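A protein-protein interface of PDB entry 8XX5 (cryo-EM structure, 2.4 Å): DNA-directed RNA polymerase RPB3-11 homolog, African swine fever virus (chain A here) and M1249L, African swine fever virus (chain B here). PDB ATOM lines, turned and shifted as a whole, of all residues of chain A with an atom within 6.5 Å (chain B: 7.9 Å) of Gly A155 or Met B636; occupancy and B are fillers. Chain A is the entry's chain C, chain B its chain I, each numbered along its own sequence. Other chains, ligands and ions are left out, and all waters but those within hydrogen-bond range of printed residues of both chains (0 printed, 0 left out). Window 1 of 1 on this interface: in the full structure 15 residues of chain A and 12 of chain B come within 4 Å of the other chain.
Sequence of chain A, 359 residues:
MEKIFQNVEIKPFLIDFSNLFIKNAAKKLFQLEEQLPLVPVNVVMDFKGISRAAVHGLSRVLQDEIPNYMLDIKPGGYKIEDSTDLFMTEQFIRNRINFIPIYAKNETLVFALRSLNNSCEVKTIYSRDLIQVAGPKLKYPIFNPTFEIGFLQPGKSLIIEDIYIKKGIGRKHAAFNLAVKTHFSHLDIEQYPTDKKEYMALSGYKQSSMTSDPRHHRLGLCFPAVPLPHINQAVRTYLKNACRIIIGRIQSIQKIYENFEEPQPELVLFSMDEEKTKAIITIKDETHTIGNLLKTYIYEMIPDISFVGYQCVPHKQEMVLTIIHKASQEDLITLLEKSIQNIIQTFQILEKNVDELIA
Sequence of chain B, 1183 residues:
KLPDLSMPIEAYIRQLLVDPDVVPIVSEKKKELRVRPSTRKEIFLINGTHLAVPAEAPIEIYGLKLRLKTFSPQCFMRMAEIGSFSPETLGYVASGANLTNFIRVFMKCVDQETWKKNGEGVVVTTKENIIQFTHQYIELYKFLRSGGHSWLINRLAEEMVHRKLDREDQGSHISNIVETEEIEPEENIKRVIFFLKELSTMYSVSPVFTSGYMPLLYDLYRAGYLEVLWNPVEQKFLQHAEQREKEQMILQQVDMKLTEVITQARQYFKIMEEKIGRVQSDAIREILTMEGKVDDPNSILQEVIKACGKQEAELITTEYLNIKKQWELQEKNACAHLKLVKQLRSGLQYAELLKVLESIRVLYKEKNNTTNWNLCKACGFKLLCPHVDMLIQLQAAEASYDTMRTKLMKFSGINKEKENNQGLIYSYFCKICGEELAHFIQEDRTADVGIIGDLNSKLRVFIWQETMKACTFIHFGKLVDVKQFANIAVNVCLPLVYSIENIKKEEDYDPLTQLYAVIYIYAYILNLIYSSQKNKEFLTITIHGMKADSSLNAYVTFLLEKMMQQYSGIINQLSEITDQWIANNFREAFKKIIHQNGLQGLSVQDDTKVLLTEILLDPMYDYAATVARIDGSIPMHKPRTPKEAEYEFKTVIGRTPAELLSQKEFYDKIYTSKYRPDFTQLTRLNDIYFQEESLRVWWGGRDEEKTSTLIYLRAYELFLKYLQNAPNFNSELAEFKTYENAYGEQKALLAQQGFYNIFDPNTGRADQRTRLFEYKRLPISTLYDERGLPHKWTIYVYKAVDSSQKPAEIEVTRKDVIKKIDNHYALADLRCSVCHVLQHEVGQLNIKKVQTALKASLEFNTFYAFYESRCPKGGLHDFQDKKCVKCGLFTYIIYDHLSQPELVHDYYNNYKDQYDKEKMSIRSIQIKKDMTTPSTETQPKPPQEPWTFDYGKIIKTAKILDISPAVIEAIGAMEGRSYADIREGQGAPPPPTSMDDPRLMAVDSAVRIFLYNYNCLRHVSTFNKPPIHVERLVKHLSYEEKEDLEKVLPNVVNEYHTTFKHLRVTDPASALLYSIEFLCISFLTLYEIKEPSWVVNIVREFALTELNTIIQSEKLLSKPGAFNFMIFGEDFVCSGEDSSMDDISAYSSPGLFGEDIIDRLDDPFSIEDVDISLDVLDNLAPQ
Printed residues of chain A that touch a printed residue of chain B: Asp A82, Thr A84, Leu A116, Asn A117, Asn A118, Ser A119, Cys A120, Pro A154, Gly A155, Lys A156 and Ser A157. Of the 17 printed residues of chain B, 7 touch a printed residue of chain A. Among the printed residues, 20 pairs touch across the chains. Among the printed residues, no Asp or Glu carboxylate lies within 4 Å of a Lys or Arg side-chain nitrogen of the other chain.
O of Ile B630 sits close to O of Asn A118, at 3.2 Å. O of Gly A155 lies close to SD of Met B636 (3.5 Å). O of Pro A154 lies within hydrogen-bond range of OG1 of Thr B626.
Of chain B, only Thr B626, Arg B629, Ile B630 and Met B636 come within 4 Å of Gly A155. Of the printed residues of chain A, Met B636 touches Thr A84 (3.2 Å), Leu A116 (3.7 Å), Asn A117 (3.3 Å), Gly A155 (3.5 Å), Lys A156 (3.5 Å) and Ser A157 (3.7 Å). Printed residues of chain B within 4 Å of Asn A118: Ile B630. Printed residues of chain B within 4 Å of Ser A119: Ile B630 (3.5 Å). Of the printed residues of chain A, Ile B630 touches Asn A118 (3.2 Å), Ser A119 (3.5 Å), Cys A120 (3.7 Å), Pro A154 (3.7 Å) and Gly A155 (3.5 Å). Printed residues of chain A within 4 Å of Tyr B712: Cys A120 (3.8 Å) and Pro A154 (3.9 Å). Printed residues of chain B within 4 Å of Lys A156: Met B636 (3.5 Å). Gly B632 touches none of the printed residues of chain A. Ser A115 touches none of the printed residues of chain B. The nearest residue of chain B that does not touch Gly A155 is Tyr B712 (5.9 Å). The nearest printed residue of chain A that does not touch Thr B626 is Lys A156 (4.1 Å).
Asp A82 touches His B637 (OD2 to CB, 3.96 Å). Arg B629 touches Thr A84 (NH1 to CG2, 3.9 Å). Met B636 touches Thr A84. CG2 of Thr A84 touches CA of His B637 (3.9 Å). Thr A84 touches Lys B638. CB of Cys A120 touches CB of Tyr B712 (3.8 Å). CD1 of Ile B630 touches CB of Pro A154, at 3.7 Å. Gly A155 touches Thr B626. CD of Arg B629 touches O of Gly A155, at 3.9 Å. OG of Ser A157 touches O of Met B636 (3.7 Å).
The side-chain amide nitrogen of Asn A117 is in hydrogen-bond range of the backbone carbonyl oxygen of Glu A121 (2.6 Å). The backbone carbonyl oxygen (O) of Asp A82 lies within hydrogen-bond range of the side-chain hydroxyl (OG) of Ser A157. N of Ser A157 is in hydrogen-bond range of OG1 of Thr A84 (2.7 Å). O of Gln A153 is in hydrogen-bond range of ND2 of Asn A117. The guanidinium group (NE) of Arg B629 lies close to the backbone carbonyl oxygen (O) of Pro B635 (3.4 Å). The backbone NH of Gly A155 is in hydrogen-bond range of the backbone carbonyl oxygen of Asn A117.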
ATOM      1  N   ASP A  82       1.075   2.092  -1.647  1.00  0.00           N
ATOM      2  CA  ASP A  82       2.470   1.677  -1.715  1.00  0.00           C
ATOM      3  C   ASP A  82       3.298   2.102  -0.510  1.00  0.00           C
ATOM      4  O   ASP A  82       4.338   1.491  -0.252  1.00  0.00           O
ATOM      5  CB  ASP A  82       3.123   2.230  -2.985  1.00  0.00           C
ATOM      6  CG  ASP A  82       2.946   1.314  -4.178  1.00  0.00           C
ATOM      7  OD1 ASP A  82       1.835   1.283  -4.745  1.00  0.00           O
ATOM      8  OD2 ASP A  82       3.920   0.626  -4.549  1.00  0.00           O
ATOM      9  N   THR A  84       4.089   1.650   2.762  1.00  0.00           N
ATOM     10  CA  THR A  84       3.848   0.693   3.832  1.00  0.00           C
ATOM     11  C   THR A  84       4.324   1.192   5.188  1.00  0.00           C
ATOM     12  O   THR A  84       3.911   0.638   6.212  1.00  0.00           O
ATOM     13  CB  THR A  84       4.528  -0.640   3.516  1.00  0.00           C
ATOM     14  OG1 THR A  84       5.854  -0.400   3.032  1.00  0.00           O
ATOM     15  CG2 THR A  84       3.745  -1.395   2.459  1.00  0.00           C
ATOM     16  N   SER A 115      11.402   5.287  -2.022  1.00  0.00           N
ATOM     17  CA  SER A 115      12.351   4.698  -1.090  1.00  0.00           C
ATOM     18  C   SER A 115      11.776   3.390  -0.567  1.00  0.00           C
ATOM     19  O   SER A 115      10.718   3.383   0.069  1.00  0.00           O
ATOM     20  CB  SER A 115      12.658   5.653   0.063  1.00  0.00           C
ATOM     21  OG  SER A 115      11.490   6.333   0.486  1.00  0.00           O
ATOM     22  N   LEU A 116      12.474   2.291  -0.839  1.00  0.00           N
ATOM     23  CA  LEU A 116      12.066   0.962  -0.407  1.00  0.00           C
ATOM     24  C   LEU A 116      13.165   0.388   0.472  1.00  0.00           C
ATOM     25  O   LEU A 116      14.310   0.255   0.029  1.00  0.00           O
ATOM     26  CB  LEU A 116      11.802   0.053  -1.608  1.00  0.00           C
ATOM     27  CG  LEU A 116      10.400   0.118  -2.218  1.00  0.00           C
ATOM     28  CD1 LEU A 116      10.286   1.283  -3.184  1.00  0.00           C
ATOM     29  CD2 LEU A 116      10.060  -1.188  -2.912  1.00  0.00           C
ATOM     30  N   ASN A 117      12.819   0.054   1.710  1.00  0.00           N
ATOM     31  CA  ASN A 117      13.770  -0.509   2.663  1.00  0.00           C
ATOM     32  C   ASN A 117      13.574  -2.018   2.689  1.00  0.00           C
ATOM     33  O   ASN A 117      12.723  -2.534   3.418  1.00  0.00           O
ATOM     34  CB  ASN A 117      13.582   0.101   4.047  1.00  0.00           C
ATOM     35  CG  ASN A 117      14.695  -0.271   5.000  1.00  0.00           C
ATOM     36  OD1 ASN A 117      15.748  -0.749   4.584  1.00  0.00           O
ATOM     37  ND2 ASN A 117      14.467  -0.059   6.287  1.00  0.00           N
ATOM     38  N   ASN A 118      14.368  -2.730   1.890  1.00  0.00           N
ATOM     39  CA  ASN A 118      14.353  -4.186   1.865  1.00  0.00           C
ATOM     40  C   ASN A 118      15.470  -4.781   2.714  1.00  0.00           C
ATOM     41  O   ASN A 118      15.998  -5.849   2.392  1.00  0.00           O
ATOM     42  CB  ASN A 118      14.439  -4.695   0.426  1.00  0.00           C
ATOM     43  CG  ASN A 118      15.715  -4.268  -0.267  1.00  0.00           C
ATOM     44  OD1 ASN A 118      16.076  -3.091  -0.258  1.00  0.00           O
ATOM     45  ND2 ASN A 118      16.405  -5.224  -0.874  1.00  0.00           N
ATOM     46  N   SER A 119      15.842  -4.102   3.793  1.00  0.00           N
ATOM     47  CA  SER A 119      16.874  -4.553   4.710  1.00  0.00           C
ATOM     48  C   SER A 119      16.325  -4.571   6.129  1.00  0.00           C
ATOM     49  O   SER A 119      15.215  -4.107   6.399  1.00  0.00           O
ATOM     50  CB  SER A 119      18.115  -3.655   4.628  1.00  0.00           C
ATOM     51  OG  SER A 119      18.013  -2.559   5.518  1.00  0.00           O
ATOM     52  N   CYS A 120      17.122  -5.114   7.044  1.00  0.00           N
ATOM     53  CA  CYS A 120      16.724  -5.240   8.439  1.00  0.00           C
ATOM     54  C   CYS A 120      17.083  -4.019   9.274  1.00  0.00           C
ATOM     55  O   CYS A 120      16.805  -4.007  10.476  1.00  0.00           O
ATOM     56  CB  CYS A 120      17.361  -6.490   9.056  1.00  0.00           C
ATOM     57  SG  CYS A 120      17.126  -7.999   8.095  1.00  0.00           S
ATOM     58  N   GLU A 121      17.689  -3.001   8.674  1.00  0.00           N
ATOM     59  CA  GLU A 121      18.037  -1.776   9.374  1.00  0.00           C
ATOM     60  C   GLU A 121      17.039  -0.673   9.041  1.00  0.00           C
ATOM     61  O   GLU A 121      16.350  -0.711   8.020  1.00  0.00           O
ATOM     62  CB  GLU A 121      19.450  -1.320   9.008  1.00  0.00           C
ATOM     63  CG  GLU A 121      20.505  -2.404   9.112  1.00  0.00           C
ATOM     64  CD  GLU A 121      21.416  -2.445   7.899  1.00  0.00           C
ATOM     65  OE1 GLU A 121      21.171  -1.679   6.943  1.00  0.00           O
ATOM     66  OE2 GLU A 121      22.378  -3.242   7.902  1.00  0.00           O
ATOM     67  N   LEU A 152      12.741   4.842   7.313  1.00  0.00           N
ATOM     68  CA  LEU A 152      11.888   3.703   7.006  1.00  0.00           C
ATOM     69  C   LEU A 152      12.216   2.547   7.937  1.00  0.00           C
ATOM     70  O   LEU A 152      13.384   2.177   8.087  1.00  0.00           O
ATOM     71  CB  LEU A 152      12.061   3.264   5.552  1.00  0.00           C
ATOM     72  CG  LEU A 152      11.490   4.181   4.472  1.00  0.00           C
ATOM     73  CD1 LEU A 152      11.971   3.740   3.108  1.00  0.00           C
ATOM     74  CD2 LEU A 152       9.978   4.201   4.528  1.00  0.00           C
ATOM     75  N   GLN A 153      11.184   1.979   8.554  1.00  0.00           N
ATOM     76  CA  GLN A 153      11.348   0.755   9.311  1.00  0.00           C
ATOM     77  C   GLN A 153      11.719  -0.383   8.362  1.00  0.00           C
ATOM     78  O   GLN A 153      11.447  -0.312   7.162  1.00  0.00           O
ATOM     79  CB  GLN A 153      10.064   0.419  10.065  1.00  0.00           C
ATOM     80  CG  GLN A 153       9.694   1.404  11.159  1.00  0.00           C
ATOM     81  CD  GLN A 153      10.854   1.730  12.075  1.00  0.00           C
ATOM     82  OE1 GLN A 153      11.494   0.837  12.627  1.00  0.00           O
ATOM     83  NE2 GLN A 153      11.127   3.017  12.248  1.00  0.00           N
ATOM     84  N   PRO A 154      12.364  -1.432   8.872  1.00  0.00           N
ATOM     85  CA  PRO A 154      12.720  -2.562   8.007  1.00  0.00           C
ATOM     86  C   PRO A 154      11.498  -3.136   7.306  1.00  0.00           C
ATOM     87  O   PRO A 154      10.437  -3.314   7.907  1.00  0.00           O
ATOM     88  CB  PRO A 154      13.337  -3.570   8.981  1.00  0.00           C
ATOM     89  CG  PRO A 154      13.858  -2.735  10.089  1.00  0.00           C
ATOM     90  CD  PRO A 154      12.908  -1.589  10.232  1.00  0.00           C
ATOM     91  N   GLY A 155      11.657  -3.419   6.014  1.00  0.00           N
ATOM     92  CA  GLY A 155      10.573  -3.952   5.215  1.00  0.00           C
ATOM     93  C   GLY A 155       9.509  -2.957   4.819  1.00  0.00           C
ATOM     94  O   GLY A 155       8.461  -3.369   4.311  1.00  0.00           O
ATOM     95  N   LYS A 156       9.737  -1.664   5.025  1.00  0.00           N
ATOM     96  CA  LYS A 156       8.748  -0.637   4.743  1.00  0.00           C
ATOM     97  C   LYS A 156       9.218   0.261   3.607  1.00  0.00           C
ATOM     98  O   LYS A 156      10.415   0.401   3.346  1.00  0.00           O
ATOM     99  CB  LYS A 156       8.459   0.203   5.990  1.00  0.00           C
ATOM    100  CG  LYS A 156       8.024  -0.613   7.192  1.00  0.00           C
ATOM    101  CD  LYS A 156       6.567  -1.013   7.089  1.00  0.00           C
ATOM    102  CE  LYS A 156       6.321  -2.366   7.724  1.00  0.00           C
ATOM    103  NZ  LYS A 156       5.599  -2.243   9.018  1.00  0.00           N
ATOM    104  N   SER A 157       8.251   0.871   2.930  1.00  0.00           N
ATOM    105  CA  SER A 157       8.520   1.718   1.780  1.00  0.00           C
ATOM    106  C   SER A 157       7.736   3.015   1.899  1.00  0.00           C
ATOM    107  O   SER A 157       6.718   3.095   2.591  1.00  0.00           O
ATOM    108  CB  SER A 157       8.163   1.013   0.467  1.00  0.00           C
ATOM    109  OG  SER A 157       6.999   0.220   0.613  1.00  0.00           O
ATOM    110  N   ALA B 625       5.155 -11.071   7.746  1.00  0.00           N
ATOM    111  CA  ALA B 625       5.022 -10.401   6.460  1.00  0.00           C
ATOM    112  C   ALA B 625       6.165  -9.428   6.216  1.00  0.00           C
ATOM    113  O   ALA B 625       6.708  -9.373   5.109  1.00  0.00           O
ATOM    114  CB  ALA B 625       3.677  -9.680   6.384  1.00  0.00           C
ATOM    115  N   THR B 626       6.547  -8.647   7.228  1.00  0.00           N
ATOM    116  CA  THR B 626       7.663  -7.728   7.033  1.00  0.00           C
ATOM    117  C   THR B 626       8.983  -8.479   6.906  1.00  0.00           C
ATOM    118  O   THR B 626       9.872  -8.038   6.169  1.00  0.00           O
ATOM    119  CB  THR B 626       7.722  -6.688   8.158  1.00  0.00           C
ATOM    120  OG1 THR B 626       8.686  -5.682   7.826  1.00  0.00           O
ATOM    121  CG2 THR B 626       8.106  -7.312   9.479  1.00  0.00           C
ATOM    122  N   VAL B 627       9.121  -9.624   7.578  1.00  0.00           N
ATOM    123  CA  VAL B 627      10.318 -10.440   7.385  1.00  0.00           C
ATOM    124  C   VAL B 627      10.380 -10.964   5.954  1.00  0.00           C
ATOM    125  O   VAL B 627      11.439 -10.949   5.315  1.00  0.00           O
ATOM    126  CB  VAL B 627      10.359 -11.580   8.418  1.00  0.00           C
ATOM    127  CG1 VAL B 627      11.404 -12.610   8.034  1.00  0.00           C
ATOM    128  CG2 VAL B 627      10.652 -11.019   9.795  1.00  0.00           C
ATOM    129  N   ALA B 628       9.244 -11.426   5.426  1.00  0.00           N
ATOM    130  CA  ALA B 628       9.201 -11.886   4.041  1.00  0.00           C
ATOM    131  C   ALA B 628       9.485 -10.748   3.068  1.00  0.00           C
ATOM    132  O   ALA B 628      10.158 -10.945   2.050  1.00  0.00           O
ATOM    133  CB  ALA B 628       7.844 -12.522   3.744  1.00  0.00           C
ATOM    134  N   ARG B 629       8.969  -9.553   3.360  1.00  0.00           N
ATOM    135  CA  ARG B 629       9.240  -8.394   2.517  1.00  0.00           C
ATOM    136  C   ARG B 629      10.722  -8.053   2.511  1.00  0.00           C
ATOM    137  O   ARG B 629      11.285  -7.711   1.464  1.00  0.00           O
ATOM    138  CB  ARG B 629       8.418  -7.198   2.993  1.00  0.00           C
ATOM    139  CG  ARG B 629       7.166  -6.949   2.183  1.00  0.00           C
ATOM    140  CD  ARG B 629       6.138  -6.177   2.981  1.00  0.00           C
ATOM    141  NE  ARG B 629       4.791  -6.677   2.742  1.00  0.00           N
ATOM    142  CZ  ARG B 629       3.686  -6.101   3.196  1.00  0.00           C
ATOM    143  NH1 ARG B 629       3.731  -4.997   3.921  1.00  0.00           N
ATOM    144  NH2 ARG B 629       2.508  -6.649   2.915  1.00  0.00           N
ATOM    145  N   ILE B 630      11.369  -8.126   3.675  1.00  0.00           N
ATOM    146  CA  ILE B 630      12.813  -7.920   3.739  1.00  0.00           C
ATOM    147  C   ILE B 630      13.529  -8.972   2.903  1.00  0.00           C
ATOM    148  O   ILE B 630      14.447  -8.665   2.134  1.00  0.00           O
ATOM    149  CB  ILE B 630      13.293  -7.937   5.201  1.00  0.00           C
ATOM    150  CG1 ILE B 630      12.839  -6.674   5.929  1.00  0.00           C
ATOM    151  CG2 ILE B 630      14.805  -8.078   5.268  1.00  0.00           C
ATOM    152  CD1 ILE B 630      12.721  -6.848   7.422  1.00  0.00           C
ATOM    153  N   ASP B 631      13.110 -10.231   3.034  1.00  0.00           N
ATOM    154  CA  ASP B 631      13.705 -11.315   2.263  1.00  0.00           C
ATOM    155  C   ASP B 631      13.270 -11.319   0.804  1.00  0.00           C
ATOM    156  O   ASP B 631      13.858 -12.052   0.003  1.00  0.00           O
ATOM    157  CB  ASP B 631      13.365 -12.661   2.906  1.00  0.00           C
ATOM    158  CG  ASP B 631      14.198 -12.944   4.140  1.00  0.00           C
ATOM    159  OD1 ASP B 631      13.945 -12.315   5.187  1.00  0.00           O
ATOM    160  OD2 ASP B 631      15.106 -13.797   4.065  1.00  0.00           O
ATOM    161  N   GLY B 632      12.263 -10.529   0.441  1.00  0.00           N
ATOM    162  CA  GLY B 632      11.828 -10.438  -0.938  1.00  0.00           C
ATOM    163  C   GLY B 632      10.870 -11.513  -1.395  1.00  0.00           C
ATOM    164  O   GLY B 632      10.588 -11.594  -2.596  1.00  0.00           O
ATOM    165  N   SER B 633      10.358 -12.343  -0.486  1.00  0.00           N
ATOM    166  CA  SER B 633       9.436 -13.403  -0.875  1.00  0.00           C
ATOM    167  C   SER B 633       8.044 -12.884  -1.207  1.00  0.00           C
ATOM    168  O   SER B 633       7.283 -13.585  -1.882  1.00  0.00           O
ATOM    169  CB  SER B 633       9.343 -14.453   0.232  1.00  0.00           C
ATOM    170  OG  SER B 633      10.630 -14.877   0.640  1.00  0.00           O
ATOM    171  N   ILE B 634       7.692 -11.688  -0.749  1.00  0.00           N
ATOM    172  CA  ILE B 634       6.403 -11.081  -1.075  1.00  0.00           C
ATOM    173  C   ILE B 634       6.650  -9.653  -1.539  1.00  0.00           C
ATOM    174  O   ILE B 634       7.691  -9.054  -1.222  1.00  0.00           O
ATOM    175  CB  ILE B 634       5.430 -11.120   0.129  1.00  0.00           C
ATOM    176  CG1 ILE B 634       6.015 -10.373   1.326  1.00  0.00           C
ATOM    177  CG2 ILE B 634       5.091 -12.553   0.501  1.00  0.00           C
ATOM    178  CD1 ILE B 634       5.007 -10.114   2.420  1.00  0.00           C
ATOM    179  N   PRO B 635       5.724  -9.084  -2.312  1.00  0.00           N
ATOM    180  CA  PRO B 635       5.900  -7.700  -2.768  1.00  0.00           C
ATOM    181  C   PRO B 635       5.977  -6.729  -1.599  1.00  0.00           C
ATOM    182  O   PRO B 635       5.347  -6.919  -0.558  1.00  0.00           O
ATOM    183  CB  PRO B 635       4.655  -7.445  -3.623  1.00  0.00           C
ATOM    184  CG  PRO B 635       4.197  -8.792  -4.040  1.00  0.00           C
ATOM    185  CD  PRO B 635       4.532  -9.711  -2.909  1.00  0.00           C
ATOM    186  N   MET B 636       6.769  -5.673  -1.790  1.00  0.00           N
ATOM    187  CA  MET B 636       6.992  -4.697  -0.731  1.00  0.00           C
ATOM    188  C   MET B 636       5.740  -3.901  -0.392  1.00  0.00           C
ATOM    189  O   MET B 636       5.684  -3.288   0.678  1.00  0.00           O
ATOM    190  CB  MET B 636       8.120  -3.745  -1.129  1.00  0.00           C
ATOM    191  CG  MET B 636       9.498  -4.202  -0.690  1.00  0.00           C
ATOM    192  SD  MET B 636       9.764  -4.001   1.081  1.00  0.00           S
ATOM    193  CE  MET B 636      10.312  -2.300   1.143  1.00  0.00           C
ATOM    194  N   HIS B 637       4.743  -3.894  -1.268  1.00  0.00           N
ATOM    195  CA  HIS B 637       3.511  -3.151  -1.051  1.00  0.00           C
ATOM    196  C   HIS B 637       2.439  -4.052  -0.450  1.00  0.00           C
ATOM    197  O   HIS B 637       2.495  -5.279  -0.547  1.00  0.00           O
ATOM    198  CB  HIS B 637       3.007  -2.548  -2.365  1.00  0.00           C
ATOM    199  CG  HIS B 637       2.840  -3.552  -3.463  1.00  0.00           C
ATOM    200  ND1 HIS B 637       1.733  -4.368  -3.562  1.00  0.00           N
ATOM    201  CD2 HIS B 637       3.640  -3.876  -4.505  1.00  0.00           C
ATOM    202  CE1 HIS B 637       1.859  -5.149  -4.620  1.00  0.00           C
ATOM    203  NE2 HIS B 637       3.007  -4.871  -5.209  1.00  0.00           N
ATOM    204  N   LYS B 638       1.455  -3.419   0.183  1.00  0.00           N
ATOM    205  CA  LYS B 638       0.298  -4.154   0.660  1.00  0.00           C
ATOM    206  C   LYS B 638      -0.531  -4.641  -0.528  1.00  0.00           C
ATOM    207  O   LYS B 638      -0.572  -3.987  -1.573  1.00  0.00           O
ATOM    208  CB  LYS B 638      -0.557  -3.282   1.576  1.00  0.00           C
ATOM    209  CG  LYS B 638       0.231  -2.260   2.375  1.00  0.00           C
ATOM    210  CD  LYS B 638      -0.627  -1.618   3.452  1.00  0.00           C
ATOM    211  CE  LYS B 638      -1.151  -0.263   3.010  1.00  0.00           C
ATOM    212  NZ  LYS B 638      -0.055   0.734   2.879  1.00  0.00           N
ATOM    213  N   PRO B 639      -1.185  -5.796  -0.397  1.00  0.00           N
ATOM    214  CA  PRO B 639      -1.933  -6.348  -1.533  1.00  0.00           C
ATOM    215  C   PRO B 639      -3.026  -5.401  -2.006  1.00  0.00           C
ATOM    216  O   PRO B 639      -3.709  -4.756  -1.208  1.00  0.00           O
ATOM    217  CB  PRO B 639      -2.520  -7.649  -0.973  1.00  0.00           C
ATOM    218  CG  PRO B 639      -1.679  -7.983   0.205  1.00  0.00           C
ATOM    219  CD  PRO B 639      -1.229  -6.679   0.780  1.00  0.00           C
ATOM    220  N   GLU B 648       0.028 -13.671  -0.434  1.00  0.00           N
ATOM    221  CA  GLU B 648       0.720 -13.233   0.774  1.00  0.00           C
ATOM    222  C   GLU B 648       0.355 -14.111   1.961  1.00  0.00           C
ATOM    223  O   GLU B 648       1.225 -14.492   2.751  1.00  0.00           O
ATOM    224  CB  GLU B 648       0.388 -11.770   1.066  1.00  0.00           C
ATOM    225  CG  GLU B 648       1.362 -11.092   2.015  1.00  0.00           C
ATOM    226  CD  GLU B 648       0.794  -9.828   2.635  1.00  0.00           C
ATOM    227  OE1 GLU B 648       0.959  -8.744   2.038  1.00  0.00           O
ATOM    228  OE2 GLU B 648       0.185  -9.918   3.721  1.00  0.00           O
ATOM    229  N   TYR B 712      17.865  -8.115  14.413  1.00  0.00           N
ATOM    230  CA  TYR B 712      16.501  -8.206  13.898  1.00  0.00           C
ATOM    231  C   TYR B 712      16.139  -9.642  13.535  1.00  0.00           C
ATOM    232  O   TYR B 712      15.071 -10.147  13.910  1.00  0.00           O
ATOM    233  CB  TYR B 712      16.356  -7.290  12.683  1.00  0.00           C
ATOM    234  CG  TYR B 712      14.932  -7.015  12.266  1.00  0.00           C
ATOM    235  CD1 TYR B 712      14.229  -5.943  12.796  1.00  0.00           C
ATOM    236  CD2 TYR B 712      14.293  -7.821  11.336  1.00  0.00           C
ATOM    237  CE1 TYR B 712      12.930  -5.687  12.415  1.00  0.00           C
ATOM    238  CE2 TYR B 712      12.995  -7.573  10.952  1.00  0.00           C
ATOM    239  CZ  TYR B 712      12.318  -6.505  11.493  1.00  0.00           C
ATOM    240  OH  TYR B 712      11.022  -6.257  11.109  1.00  0.00           O
